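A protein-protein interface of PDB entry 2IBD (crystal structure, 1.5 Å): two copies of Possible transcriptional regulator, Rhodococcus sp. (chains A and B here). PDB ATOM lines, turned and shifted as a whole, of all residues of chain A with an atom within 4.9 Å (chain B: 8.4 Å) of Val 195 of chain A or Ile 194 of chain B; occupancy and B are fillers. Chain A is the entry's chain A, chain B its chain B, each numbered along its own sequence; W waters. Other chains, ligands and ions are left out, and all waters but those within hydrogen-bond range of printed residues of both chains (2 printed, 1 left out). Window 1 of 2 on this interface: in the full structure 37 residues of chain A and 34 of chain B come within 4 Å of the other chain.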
ATOM      1  N   ARG A 153     -27.549 -15.714 -32.388  1.00  0.00           N
ATOM      2  CA  ARG A 153     -28.227 -16.321 -33.534  1.00  0.00           C
ATOM      3  C   ARG A 153     -29.709 -16.036 -33.492  1.00  0.00           C
ATOM      4  O   ARG A 153     -30.299 -16.002 -32.428  1.00  0.00           O
ATOM      5  CB  ARG A 153     -28.027 -17.838 -33.533  1.00  0.00           C
ATOM      6  CG  ARG A 153     -26.638 -18.255 -33.940  1.00  0.00           C
ATOM      7  CD  ARG A 153     -26.356 -19.682 -33.437  1.00  0.00           C
ATOM      8  NE  ARG A 153     -27.356 -20.600 -33.955  1.00  0.00           N
ATOM      9  CZ  ARG A 153     -27.464 -21.864 -33.591  1.00  0.00           C
ATOM     10  NH1 ARG A 153     -26.666 -22.364 -32.629  1.00  0.00           N
ATOM     11  NH2 ARG A 153     -28.401 -22.602 -34.166  1.00  0.00           N
ATOM     12  N   ILE A 156     -32.427 -19.504 -32.594  1.00  0.00           N
ATOM     13  CA  ILE A 156     -32.566 -20.134 -31.295  1.00  0.00           C
ATOM     14  C   ILE A 156     -33.673 -19.366 -30.554  1.00  0.00           C
ATOM     15  O   ILE A 156     -33.678 -18.144 -30.522  1.00  0.00           O
ATOM     16  CB  ILE A 156     -31.234 -20.099 -30.494  1.00  0.00           C
ATOM     17  CG1 ILE A 156     -30.166 -20.999 -31.146  1.00  0.00           C
ATOM     18  CG2 ILE A 156     -31.453 -20.507 -29.050  1.00  0.00           C
ATOM     19  CD1 ILE A 156     -30.492 -22.506 -31.150  1.00  0.00           C
ATOM     20  N   ALA A 161     -33.203 -20.412 -24.612  1.00  0.00           N
ATOM     21  CA  ALA A 161     -31.804 -20.022 -24.327  1.00  0.00           C
ATOM     22  C   ALA A 161     -31.715 -19.441 -22.935  1.00  0.00           C
ATOM     23  O   ALA A 161     -30.763 -19.744 -22.171  1.00  0.00           O
ATOM     24  CB  ALA A 161     -31.318 -19.038 -25.330  1.00  0.00           C
ATOM     25  N   PHE A 164     -31.914 -22.224 -20.407  1.00  0.00           N
ATOM     26  CA  PHE A 164     -30.626 -22.948 -20.339  1.00  0.00           C
ATOM     27  C   PHE A 164     -29.650 -22.175 -19.428  1.00  0.00           C
ATOM     28  O   PHE A 164     -28.986 -22.788 -18.541  1.00  0.00           O
ATOM     29  CB  PHE A 164     -30.047 -23.140 -21.739  1.00  0.00           C
ATOM     30  CG  PHE A 164     -28.649 -23.619 -21.723  1.00  0.00           C
ATOM     31  CD1 PHE A 164     -28.384 -24.965 -21.615  1.00  0.00           C
ATOM     32  CD2 PHE A 164     -27.593 -22.703 -21.795  1.00  0.00           C
ATOM     33  CE1 PHE A 164     -27.014 -25.417 -21.570  1.00  0.00           C
ATOM     34  CE2 PHE A 164     -26.296 -23.120 -21.751  1.00  0.00           C
ATOM     35  CZ  PHE A 164     -25.997 -24.458 -21.639  1.00  0.00           C
ATOM     36  N   LEU A 165     -29.535 -20.860 -19.644  1.00  0.00           N
ATOM     37  CA  LEU A 165     -28.614 -20.075 -18.813  1.00  0.00           C
ATOM     38  C   LEU A 165     -29.030 -20.086 -17.353  1.00  0.00           C
ATOM     39  O   LEU A 165     -28.201 -20.208 -16.436  1.00  0.00           O
ATOM     40  CB  LEU A 165     -28.509 -18.631 -19.326  1.00  0.00           C
ATOM     41  CG  LEU A 165     -27.828 -18.523 -20.696  1.00  0.00           C
ATOM     42  CD1 LEU A 165     -28.067 -17.092 -21.235  1.00  0.00           C
ATOM     43  CD2 LEU A 165     -26.362 -18.801 -20.673  1.00  0.00           C
ATOM     44  N   TYR A 191     -16.924 -22.377 -19.848  1.00  0.00           N
ATOM     45  CA  TYR A 191     -18.376 -22.465 -19.995  1.00  0.00           C
ATOM     46  C   TYR A 191     -18.821 -21.486 -21.106  1.00  0.00           C
ATOM     47  O   TYR A 191     -19.634 -21.826 -22.007  1.00  0.00           O
ATOM     48  CB  TYR A 191     -19.042 -22.099 -18.666  1.00  0.00           C
ATOM     49  CG  TYR A 191     -20.554 -21.917 -18.715  1.00  0.00           C
ATOM     50  CD1 TYR A 191     -21.403 -22.983 -18.391  1.00  0.00           C
ATOM     51  CD2 TYR A 191     -21.119 -20.682 -19.046  1.00  0.00           C
ATOM     52  CE1 TYR A 191     -22.796 -22.809 -18.391  1.00  0.00           C
ATOM     53  CE2 TYR A 191     -22.479 -20.499 -19.075  1.00  0.00           C
ATOM     54  CZ  TYR A 191     -23.321 -21.550 -18.731  1.00  0.00           C
ATOM     55  OH  TYR A 191     -24.684 -21.334 -18.753  1.00  0.00           O
ATOM     56  N   LEU A 192     -18.282 -20.258 -21.041  1.00  0.00           N
ATOM     57  CA  LEU A 192     -18.656 -19.259 -22.014  1.00  0.00           C
ATOM     58  C   LEU A 192     -18.208 -19.626 -23.421  1.00  0.00           C
ATOM     59  O   LEU A 192     -18.932 -19.393 -24.391  1.00  0.00           O
ATOM     60  CB  LEU A 192     -18.081 -17.889 -21.610  1.00  0.00           C
ATOM     61  CG  LEU A 192     -18.872 -17.205 -20.486  1.00  0.00           C
ATOM     62  CD1 LEU A 192     -18.016 -16.064 -19.865  1.00  0.00           C
ATOM     63  CD2 LEU A 192     -20.238 -16.723 -21.022  1.00  0.00           C
ATOM     64  N   SER A 193     -17.023 -20.211 -23.540  1.00  0.00           N
ATOM     65  CA  SER A 193     -16.541 -20.588 -24.868  1.00  0.00           C
ATOM     66  C   SER A 193     -17.456 -21.650 -25.491  1.00  0.00           C
ATOM     67  O   SER A 193     -17.775 -21.602 -26.699  1.00  0.00           O
ATOM     68  CB  SER A 193     -15.119 -21.115 -24.752  1.00  0.00           C
ATOM     69  OG  SER A 193     -14.613 -21.406 -26.032  1.00  0.00           O
ATOM     70  N   ILE A 194     -17.882 -22.601 -24.666  1.00  0.00           N
ATOM     71  CA  ILE A 194     -18.819 -23.645 -25.156  1.00  0.00           C
ATOM     72  C   ILE A 194     -20.176 -23.057 -25.544  1.00  0.00           C
ATOM     73  O   ILE A 194     -20.653 -23.239 -26.678  1.00  0.00           O
ATOM     74  CB  ILE A 194     -18.998 -24.765 -24.140  1.00  0.00           C
ATOM     75  CG1 ILE A 194     -17.687 -25.562 -24.082  1.00  0.00           C
ATOM     76  CG2 ILE A 194     -20.197 -25.654 -24.505  1.00  0.00           C
ATOM     77  CD1 ILE A 194     -17.637 -26.558 -22.920  1.00  0.00           C
ATOM     78  N   VAL A 195     -20.770 -22.320 -24.613  1.00  0.00           N
ATOM     79  CA  VAL A 195     -22.110 -21.787 -24.843  1.00  0.00           C
ATOM     80  C   VAL A 195     -22.164 -20.752 -25.967  1.00  0.00           C
ATOM     81  O   VAL A 195     -23.164 -20.710 -26.700  1.00  0.00           O
ATOM     82  CB  VAL A 195     -22.696 -21.232 -23.532  1.00  0.00           C
ATOM     83  CG1 VAL A 195     -23.951 -20.410 -23.794  1.00  0.00           C
ATOM     84  CG2 VAL A 195     -22.919 -22.418 -22.562  1.00  0.00           C
ATOM     85  N   LEU A 196     -21.134 -19.905 -26.086  1.00  0.00           N
ATOM     86  CA  LEU A 196     -21.147 -18.916 -27.167  1.00  0.00           C
ATOM     87  C   LEU A 196     -20.598 -19.414 -28.498  1.00  0.00           C
ATOM     88  O   LEU A 196     -21.159 -19.087 -29.545  1.00  0.00           O
ATOM     89  CB  LEU A 196     -20.421 -17.652 -26.744  1.00  0.00           C
ATOM     90  CG  LEU A 196     -21.203 -16.813 -25.729  1.00  0.00           C
ATOM     91  CD1 LEU A 196     -20.280 -15.929 -24.924  1.00  0.00           C
ATOM     92  CD2 LEU A 196     -22.173 -15.947 -26.520  1.00  0.00           C
ATOM     93  N   ASP A 197     -19.527 -20.208 -28.459  1.00  0.00           N
ATOM     94  CA  ASP A 197     -18.839 -20.607 -29.702  1.00  0.00           C
ATOM     95  C   ASP A 197     -18.950 -22.097 -30.050  1.00  0.00           C
ATOM     96  O   ASP A 197     -18.592 -22.496 -31.167  1.00  0.00           O
ATOM     97  CB  ASP A 197     -17.375 -20.175 -29.634  1.00  0.00           C
ATOM     98  CG  ASP A 197     -17.228 -18.673 -29.491  1.00  0.00           C
ATOM     99  OD1 ASP A 197     -18.039 -17.936 -30.112  1.00  0.00           O
ATOM    100  OD2 ASP A 197     -16.302 -18.236 -28.756  1.00  0.00           O
ATOM    101  N   GLY A 198     -19.460 -22.907 -29.114  1.00  0.00           N
ATOM    102  CA  GLY A 198     -19.756 -24.323 -29.383  1.00  0.00           C
ATOM    103  C   GLY A 198     -18.579 -25.238 -29.096  1.00  0.00           C
ATOM    104  O   GLY A 198     -17.389 -24.859 -29.242  1.00  0.00           O
ATOM    105  N   ARG B  88     -20.043 -36.666 -33.136  1.00  0.00           N
ATOM    106  CA  ARG B  88     -21.084 -35.679 -32.838  1.00  0.00           C
ATOM    107  C   ARG B  88     -22.453 -36.363 -32.768  1.00  0.00           C
ATOM    108  O   ARG B  88     -23.254 -36.068 -31.864  1.00  0.00           O
ATOM    109  CB  ARG B  88     -21.095 -34.542 -33.868  1.00  0.00           C
ATOM    110  CG  ARG B  88     -22.227 -33.555 -33.624  1.00  0.00           C
ATOM    111  CD  ARG B  88     -22.142 -32.334 -34.542  1.00  0.00           C
ATOM    112  NE  ARG B  88     -23.278 -31.456 -34.314  1.00  0.00           N
ATOM    113  CZ  ARG B  88     -23.291 -30.132 -34.444  1.00  0.00           C
ATOM    114  NH1 ARG B  88     -22.203 -29.462 -34.802  1.00  0.00           N
ATOM    115  NH2 ARG B  88     -24.406 -29.467 -34.158  1.00  0.00           N
ATOM    116  N   ARG B 153     -13.585 -29.533 -30.310  1.00  0.00           N
ATOM    117  CA  ARG B 153     -12.410 -28.656 -30.246  1.00  0.00           C
ATOM    118  C   ARG B 153     -11.291 -29.234 -29.397  1.00  0.00           C
ATOM    119  O   ARG B 153     -11.529 -29.797 -28.328  1.00  0.00           O
ATOM    120  CB  ARG B 153     -12.827 -27.306 -29.658  1.00  0.00           C
ATOM    121  CG  ARG B 153     -13.643 -26.480 -30.574  1.00  0.00           C
ATOM    122  CD  ARG B 153     -14.368 -25.424 -29.798  1.00  0.00           C
ATOM    123  NE  ARG B 153     -13.450 -24.620 -28.998  1.00  0.00           N
ATOM    124  CZ  ARG B 153     -13.845 -23.687 -28.141  1.00  0.00           C
ATOM    125  NH1 ARG B 153     -15.160 -23.454 -27.969  1.00  0.00           N
ATOM    126  NH2 ARG B 153     -12.924 -22.997 -27.465  1.00  0.00           N
ATOM    127  N   PHE B 164     -19.422 -30.220 -17.488  1.00  0.00           N
ATOM    128  CA  PHE B 164     -20.536 -29.427 -18.011  1.00  0.00           C
ATOM    129  C   PHE B 164     -21.641 -30.317 -18.580  1.00  0.00           C
ATOM    130  O   PHE B 164     -22.826 -30.099 -18.277  1.00  0.00           O
ATOM    131  CB  PHE B 164     -20.014 -28.472 -19.076  1.00  0.00           C
ATOM    132  CG  PHE B 164     -21.103 -27.816 -19.871  1.00  0.00           C
ATOM    133  CD1 PHE B 164     -21.705 -26.643 -19.421  1.00  0.00           C
ATOM    134  CD2 PHE B 164     -21.551 -28.390 -21.034  1.00  0.00           C
ATOM    135  CE1 PHE B 164     -22.707 -26.039 -20.153  1.00  0.00           C
ATOM    136  CE2 PHE B 164     -22.570 -27.797 -21.754  1.00  0.00           C
ATOM    137  CZ  PHE B 164     -23.139 -26.607 -21.312  1.00  0.00           C
ATOM    138  N   THR B 168     -25.335 -30.652 -16.531  1.00  0.00           N
ATOM    139  CA  THR B 168     -26.477 -30.036 -17.206  1.00  0.00           C
ATOM    140  C   THR B 168     -27.444 -31.024 -17.822  1.00  0.00           C
ATOM    141  O   THR B 168     -28.423 -30.611 -18.459  1.00  0.00           O
ATOM    142  CB  THR B 168     -26.024 -29.013 -18.250  1.00  0.00           C
ATOM    143  OG1 THR B 168     -25.375 -29.709 -19.318  1.00  0.00           O
ATOM    144  CG2 THR B 168     -25.068 -27.983 -17.629  1.00  0.00           C
ATOM    145  N   VAL B 187     -36.711 -29.033 -27.382  1.00  0.00           N
ATOM    146  CA  VAL B 187     -35.836 -28.551 -26.322  1.00  0.00           C
ATOM    147  C   VAL B 187     -34.433 -29.174 -26.484  1.00  0.00           C
ATOM    148  O   VAL B 187     -33.422 -28.474 -26.400  1.00  0.00           O
ATOM    149  CB  VAL B 187     -36.421 -28.861 -24.904  1.00  0.00           C
ATOM    150  CG1 VAL B 187     -35.513 -28.357 -23.813  1.00  0.00           C
ATOM    151  CG2 VAL B 187     -37.809 -28.247 -24.770  1.00  0.00           C
ATOM    152  N   ALA B 188     -34.378 -30.494 -26.702  1.00  0.00           N
ATOM    153  CA  ALA B 188     -33.094 -31.188 -26.892  1.00  0.00           C
ATOM    154  C   ALA B 188     -32.328 -30.615 -28.082  1.00  0.00           C
ATOM    155  O   ALA B 188     -31.109 -30.359 -27.997  1.00  0.00           O
ATOM    156  CB  ALA B 188     -33.325 -32.697 -27.050  1.00  0.00           C
ATOM    157  N   LYS B 189     -33.032 -30.392 -29.193  1.00  0.00           N
ATOM    158  CA  LYS B 189     -32.348 -29.921 -30.406  1.00  0.00           C
ATOM    159  C   LYS B 189     -31.761 -28.536 -30.166  1.00  0.00           C
ATOM    160  O   LYS B 189     -30.655 -28.217 -30.649  1.00  0.00           O
ATOM    161  CB  LYS B 189     -33.280 -29.891 -31.631  1.00  0.00           C
ATOM    162  CG  LYS B 189     -33.642 -31.253 -32.160  1.00  0.00           C
ATOM    163  CD  LYS B 189     -34.501 -31.157 -33.431  1.00  0.00           C
ATOM    164  CE  LYS B 189     -34.544 -32.516 -34.096  1.00  0.00           C
ATOM    165  NZ  LYS B 189     -35.577 -32.584 -35.160  1.00  0.00           N
ATOM    166  N   GLN B 190     -32.517 -27.678 -29.459  1.00  0.00           N
ATOM    167  CA  GLN B 190     -32.034 -26.319 -29.242  1.00  0.00           C
ATOM    168  C   GLN B 190     -30.856 -26.301 -28.268  1.00  0.00           C
ATOM    169  O   GLN B 190     -29.878 -25.565 -28.470  1.00  0.00           O
ATOM    170  CB  GLN B 190     -33.169 -25.366 -28.871  1.00  0.00           C
ATOM    171  CG  GLN B 190     -34.206 -25.277 -30.033  1.00  0.00           C
ATOM    172  CD  GLN B 190     -34.678 -23.871 -30.274  1.00  0.00           C
ATOM    173  OE1 GLN B 190     -34.146 -22.920 -29.697  1.00  0.00           O
ATOM    174  NE2 GLN B 190     -35.696 -23.723 -31.148  1.00  0.00           N
ATOM    175  N   TYR B 191     -30.934 -27.133 -27.246  1.00  0.00           N
ATOM    176  CA  TYR B 191     -29.839 -27.155 -26.314  1.00  0.00           C
ATOM    177  C   TYR B 191     -28.569 -27.778 -26.937  1.00  0.00           C
ATOM    178  O   TYR B 191     -27.440 -27.328 -26.648  1.00  0.00           O
ATOM    179  CB  TYR B 191     -30.316 -27.833 -25.028  1.00  0.00           C
ATOM    180  CG  TYR B 191     -31.248 -26.947 -24.223  1.00  0.00           C
ATOM    181  CD1 TYR B 191     -31.660 -25.688 -24.694  1.00  0.00           C
ATOM    182  CD2 TYR B 191     -31.731 -27.376 -22.993  1.00  0.00           C
ATOM    183  CE1 TYR B 191     -32.512 -24.870 -23.939  1.00  0.00           C
ATOM    184  CE2 TYR B 191     -32.603 -26.608 -22.240  1.00  0.00           C
ATOM    185  CZ  TYR B 191     -32.983 -25.342 -22.707  1.00  0.00           C
ATOM    186  OH  TYR B 191     -33.819 -24.575 -21.920  1.00  0.00           O
ATOM    187  N   LEU B 192     -28.741 -28.778 -27.808  1.00  0.00           N
ATOM    188  CA  LEU B 192     -27.606 -29.339 -28.551  1.00  0.00           C
ATOM    189  C   LEU B 192     -27.020 -28.313 -29.504  1.00  0.00           C
ATOM    190  O   LEU B 192     -25.796 -28.239 -29.698  1.00  0.00           O
ATOM    191  CB  LEU B 192     -28.016 -30.598 -29.327  1.00  0.00           C
ATOM    192  CG  LEU B 192     -28.091 -31.828 -28.447  1.00  0.00           C
ATOM    193  CD1 LEU B 192     -28.911 -32.966 -29.058  1.00  0.00           C
ATOM    194  CD2 LEU B 192     -26.684 -32.293 -28.121  1.00  0.00           C
ATOM    195  N   SER B 193     -27.889 -27.537 -30.143  1.00  0.00           N
ATOM    196  CA  SER B 193     -27.407 -26.498 -31.054  1.00  0.00           C
ATOM    197  C   SER B 193     -26.539 -25.454 -30.364  1.00  0.00           C
ATOM    198  O   SER B 193     -25.488 -25.055 -30.894  1.00  0.00           O
ATOM    199  CB  SER B 193     -28.577 -25.832 -31.763  1.00  0.00           C
ATOM    200  OG  SER B 193     -28.064 -24.934 -32.731  1.00  0.00           O
ATOM    201  N   ILE B 194     -26.969 -25.024 -29.172  1.00  0.00           N
ATOM    202  CA  ILE B 194     -26.174 -24.080 -28.359  1.00  0.00           C
ATOM    203  C   ILE B 194     -24.855 -24.742 -27.956  1.00  0.00           C
ATOM    204  O   ILE B 194     -23.793 -24.193 -28.180  1.00  0.00           O
ATOM    205  CB  ILE B 194     -26.967 -23.639 -27.090  1.00  0.00           C
ATOM    206  CG1 ILE B 194     -28.190 -22.814 -27.494  1.00  0.00           C
ATOM    207  CG2 ILE B 194     -26.046 -22.911 -26.088  1.00  0.00           C
ATOM    208  CD1 ILE B 194     -29.163 -22.553 -26.308  1.00  0.00           C
ATOM    209  N   VAL B 195     -24.929 -25.936 -27.364  1.00  0.00           N
ATOM    210  CA  VAL B 195     -23.711 -26.565 -26.822  1.00  0.00           C
ATOM    211  C   VAL B 195     -22.719 -26.898 -27.921  1.00  0.00           C
ATOM    212  O   VAL B 195     -21.503 -26.737 -27.716  1.00  0.00           O
ATOM    213  CB  VAL B 195     -24.068 -27.807 -25.974  1.00  0.00           C
ATOM    214  CG1 VAL B 195     -22.824 -28.680 -25.698  1.00  0.00           C
ATOM    215  CG2 VAL B 195     -24.762 -27.293 -24.698  1.00  0.00           C
ATOM    216  N   LEU B 196     -23.207 -27.376 -29.074  1.00  0.00           N
ATOM    217  CA  LEU B 196     -22.268 -27.801 -30.104  1.00  0.00           C
ATOM    218  C   LEU B 196     -21.840 -26.672 -31.034  1.00  0.00           C
ATOM    219  O   LEU B 196     -20.675 -26.609 -31.427  1.00  0.00           O
ATOM    220  CB  LEU B 196     -22.853 -28.966 -30.906  1.00  0.00           C
ATOM    221  CG  LEU B 196     -22.778 -30.279 -30.154  1.00  0.00           C
ATOM    222  CD1 LEU B 196     -23.799 -31.240 -30.701  1.00  0.00           C
ATOM    223  CD2 LEU B 196     -21.347 -30.856 -30.296  1.00  0.00           C
ATOM    224  N   ASP B 197     -22.778 -25.788 -31.394  1.00  0.00           N
ATOM    225  CA  ASP B 197     -22.499 -24.742 -32.389  1.00  0.00           C
ATOM    226  C   ASP B 197     -22.410 -23.315 -31.839  1.00  0.00           C
ATOM    227  O   ASP B 197     -21.941 -22.413 -32.543  1.00  0.00           O
ATOM    228  CB  ASP B 197     -23.516 -24.828 -33.540  1.00  0.00           C
ATOM    229  CG  ASP B 197     -23.420 -26.153 -34.299  1.00  0.00           C
ATOM    230  OD1 ASP B 197     -22.299 -26.656 -34.488  1.00  0.00           O
ATOM    231  OD2 ASP B 197     -24.473 -26.692 -34.704  1.00  0.00           O
ATOM    232  N   GLY B 198     -22.835 -23.130 -30.577  1.00  0.00           N
ATOM    233  CA  GLY B 198     -22.725 -21.836 -29.918  1.00  0.00           C
ATOM    234  C   GLY B 198     -23.924 -20.935 -30.170  1.00  0.00           C
ATOM    235  O   GLY B 198     -24.564 -20.984 -31.221  1.00  0.00           O
ATOM    236  N   LEU B 199     -24.218 -20.100 -29.180  1.00  0.00           N
ATOM    237  CA  LEU B 199     -25.271 -19.112 -29.291  1.00  0.00           C
ATOM    238  C   LEU B 199     -24.848 -17.881 -30.132  1.00  0.00           C
ATOM    239  O   LEU B 199     -25.698 -17.182 -30.663  1.00  0.00           O
ATOM    240  CB  LEU B 199     -25.650 -18.687 -27.866  1.00  0.00           C
ATOM    241  CG  LEU B 199     -26.687 -17.595 -27.693  1.00  0.00           C
ATOM    242  CD1 LEU B 199     -28.047 -18.117 -28.119  1.00  0.00           C
ATOM    243  CD2 LEU B 199     -26.723 -17.173 -26.214  1.00  0.00           C
ATOM    244  N   ALA B 200     -23.546 -17.608 -30.259  1.00  0.00           N
ATOM    245  CA  ALA B 200     -23.110 -16.414 -30.998  1.00  0.00           C
ATOM    246  C   ALA B 200     -23.365 -16.601 -32.488  1.00  0.00           C
ATOM    247  O   ALA B 200     -23.314 -17.722 -32.986  1.00  0.00           O
ATOM    248  CB  ALA B 200     -21.638 -16.166 -30.781  1.00  0.00           C
ATOM    249  N   SER B 201     -23.639 -15.506 -33.191  1.00  0.00           N
ATOM    250  CA  SER B 201     -23.783 -15.558 -34.647  1.00  0.00           C
ATOM    251  C   SER B 201     -22.431 -15.828 -35.275  1.00  0.00           C
ATOM    252  O   SER B 201     -21.397 -15.357 -34.775  1.00  0.00           O
ATOM    253  CB  SER B 201     -24.281 -14.221 -35.156  1.00  0.00           C
ATOM    254  OG  SER B 201     -25.556 -14.013 -34.645  1.00  0.00           O
HETATM  255  O   HOH W   1     -32.952 -22.119 -27.392  1.00  0.00           O
HETATM  256  O   HOH W   2     -26.862 -25.654 -34.842  1.00  0.00           O
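The guanidinium group of Arg 153 of chain A sits at hydrogen-bond distance from the side-chain hydroxyl of Ser 193 of chain B, 2.8 Å away. The guanidinium group (NH1) of Arg 153 of chain A lies within hydrogen-bond range of the backbone carbonyl oxygen (O) of Gly 198 of chain B (2.9 Å). O of Leu 199 of chain B is in hydrogen-bond range of N of Arg 153 of chain A, 2.9 Å away. The side-chain hydroxyl (OG) of Ser 201 of chain B is in hydrogen-bond range of the backbone NH (N) of Arg 153 of chain A. N of Phe 164 of chain A lies within hydrogen-bond range of OH of Tyr 191 of chain B (3.4 Å). OG of Ser 193 of chain A lies within hydrogen-bond range of NH2 of Arg 153 of chain B (2.7 Å). The backbone carbonyl oxygen (O) of Val 195 of chain A lies within hydrogen-bond range of the backbone NH (N) of Leu 199 of chain B (2.8 Å). O of Leu 196 of chain A sits at hydrogen-bond distance from N of Leu 199 of chain B, 3.2 Å away. The backbone NH (N) of Ala 200 of chain B lies within hydrogen-bond range of the backbone carbonyl oxygen (O) of Leu 196 of chain A (2.9 Å). The guanidinium group (NH1) of Arg 153 of chain B lies within hydrogen-bond range of the backbone carbonyl oxygen (O) of Gly 198 of chain A (2.9 Å).
Of chain A, only Ile 194 (3.6 Å) and Val 195 (3.7 Å) come within 4 Å of Ile 194 of chain B. Printed residues of chain A within 4 Å of Phe 164 of chain B: Phe 164 and Tyr 191. Of the printed residues of chain B, Ile 194 of chain A touches Ile 194 (3.6 Å) and Val 195 (3.6 Å). Printed residues of chain A within 4 Å of Ser 201 of chain B: Arg 153. Ala 161 of chain A touches none of the printed residues of chain B. The nearest residue of chain A that does not touch Ile 194 of chain B is Ile 156 of chain A (4.1 Å).
Ile 156 of chain A touches Gln 190 of chain B (CA to OE1, 3.6 Å). Ile 156 of chain A touches Ser 193 of chain B (CD1 to OG, 3.8 Å). O of Ile 194 of chain B touches O of Ile 194 of chain A, at 3.6 Å. O of Val 195 of chain B touches CG2 of Ile 194 of chain A (3.6 Å). Val 195 of chain A touches Gly 198 of chain B. O of Leu 196 of chain A touches CA of Gly 198 of chain B, 3.2 Å away. Asp 197 of chain A touches Asp 197 of chain B (O to O, 3.6 Å). Gly 198 of chain A touches Leu 196 of chain B. Asp 197 of chain B touches Gly 198 of chain A (C to CA, 3.8 Å). Gly 198 of chain A touches Gly 198 of chain B.
Water W2 lies within hydrogen-bond range of OG of Ser 193 of chain B (2.5 Å), OD2 of Asp 197 of chain B (2.6 Å) and NH2 of Arg 153 of chain A (3.5 Å). Water W1 bridges OE1 of Gln 190 of chain B (2.7 Å) and N of Ala 161 of chain A (3.3 Å).
Phe 164 of chain A touches Tyr 191 of chain B, and with the chains exchanged Tyr 191 of chain A touches Phe 164 of chain B. Ile 194 of chain A touches Val 195 of chain B, and with the chains exchanged Val 195 of chain A touches Ile 194 of chain B. Val 195 of chain A touches Gly 198 of chain B, and with the chains exchanged Gly 198 of chain A touches Val 195 of chain B. Gly 198 of chain B touches its own counterpart, Gly 198 of chain A. 10 positions are printed for both chains.
The backbone carbonyl oxygen (O) of Ser 193 of chain A is in hydrogen-bond range of the backbone NH (N) of Gly 198 of chain A. NH1 of Arg 88 of chain B is in salt-bridge range of OD1 of Asp 197 of chain B, at 2.8 Å. O of Phe 164 of chain B sits at hydrogen-bond distance from OG1 of Thr 168 of chain B (2.8 Å). The backbone carbonyl oxygen of Ser 193 of chain B sits at hydrogen-bond distance from the backbone NH of Gly 198 of chain B, 3.3 Å away.
Hydrophobic or aromatic side chains of chain B that line the printed part of chain A: Phe 164, Tyr 191, Ile 194, Leu 199 and Ala 200. Hydrophobic or aromatic side chains of chain A within 4 Å of the printed part of chain B: Ile 156, Phe 164, Tyr 191, Ile 194 and Val 195. Among the printed residues, no Asp or Glu carboxylate lies within 4 Å of a Lys or Arg side-chain nitrogen of the other chain.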
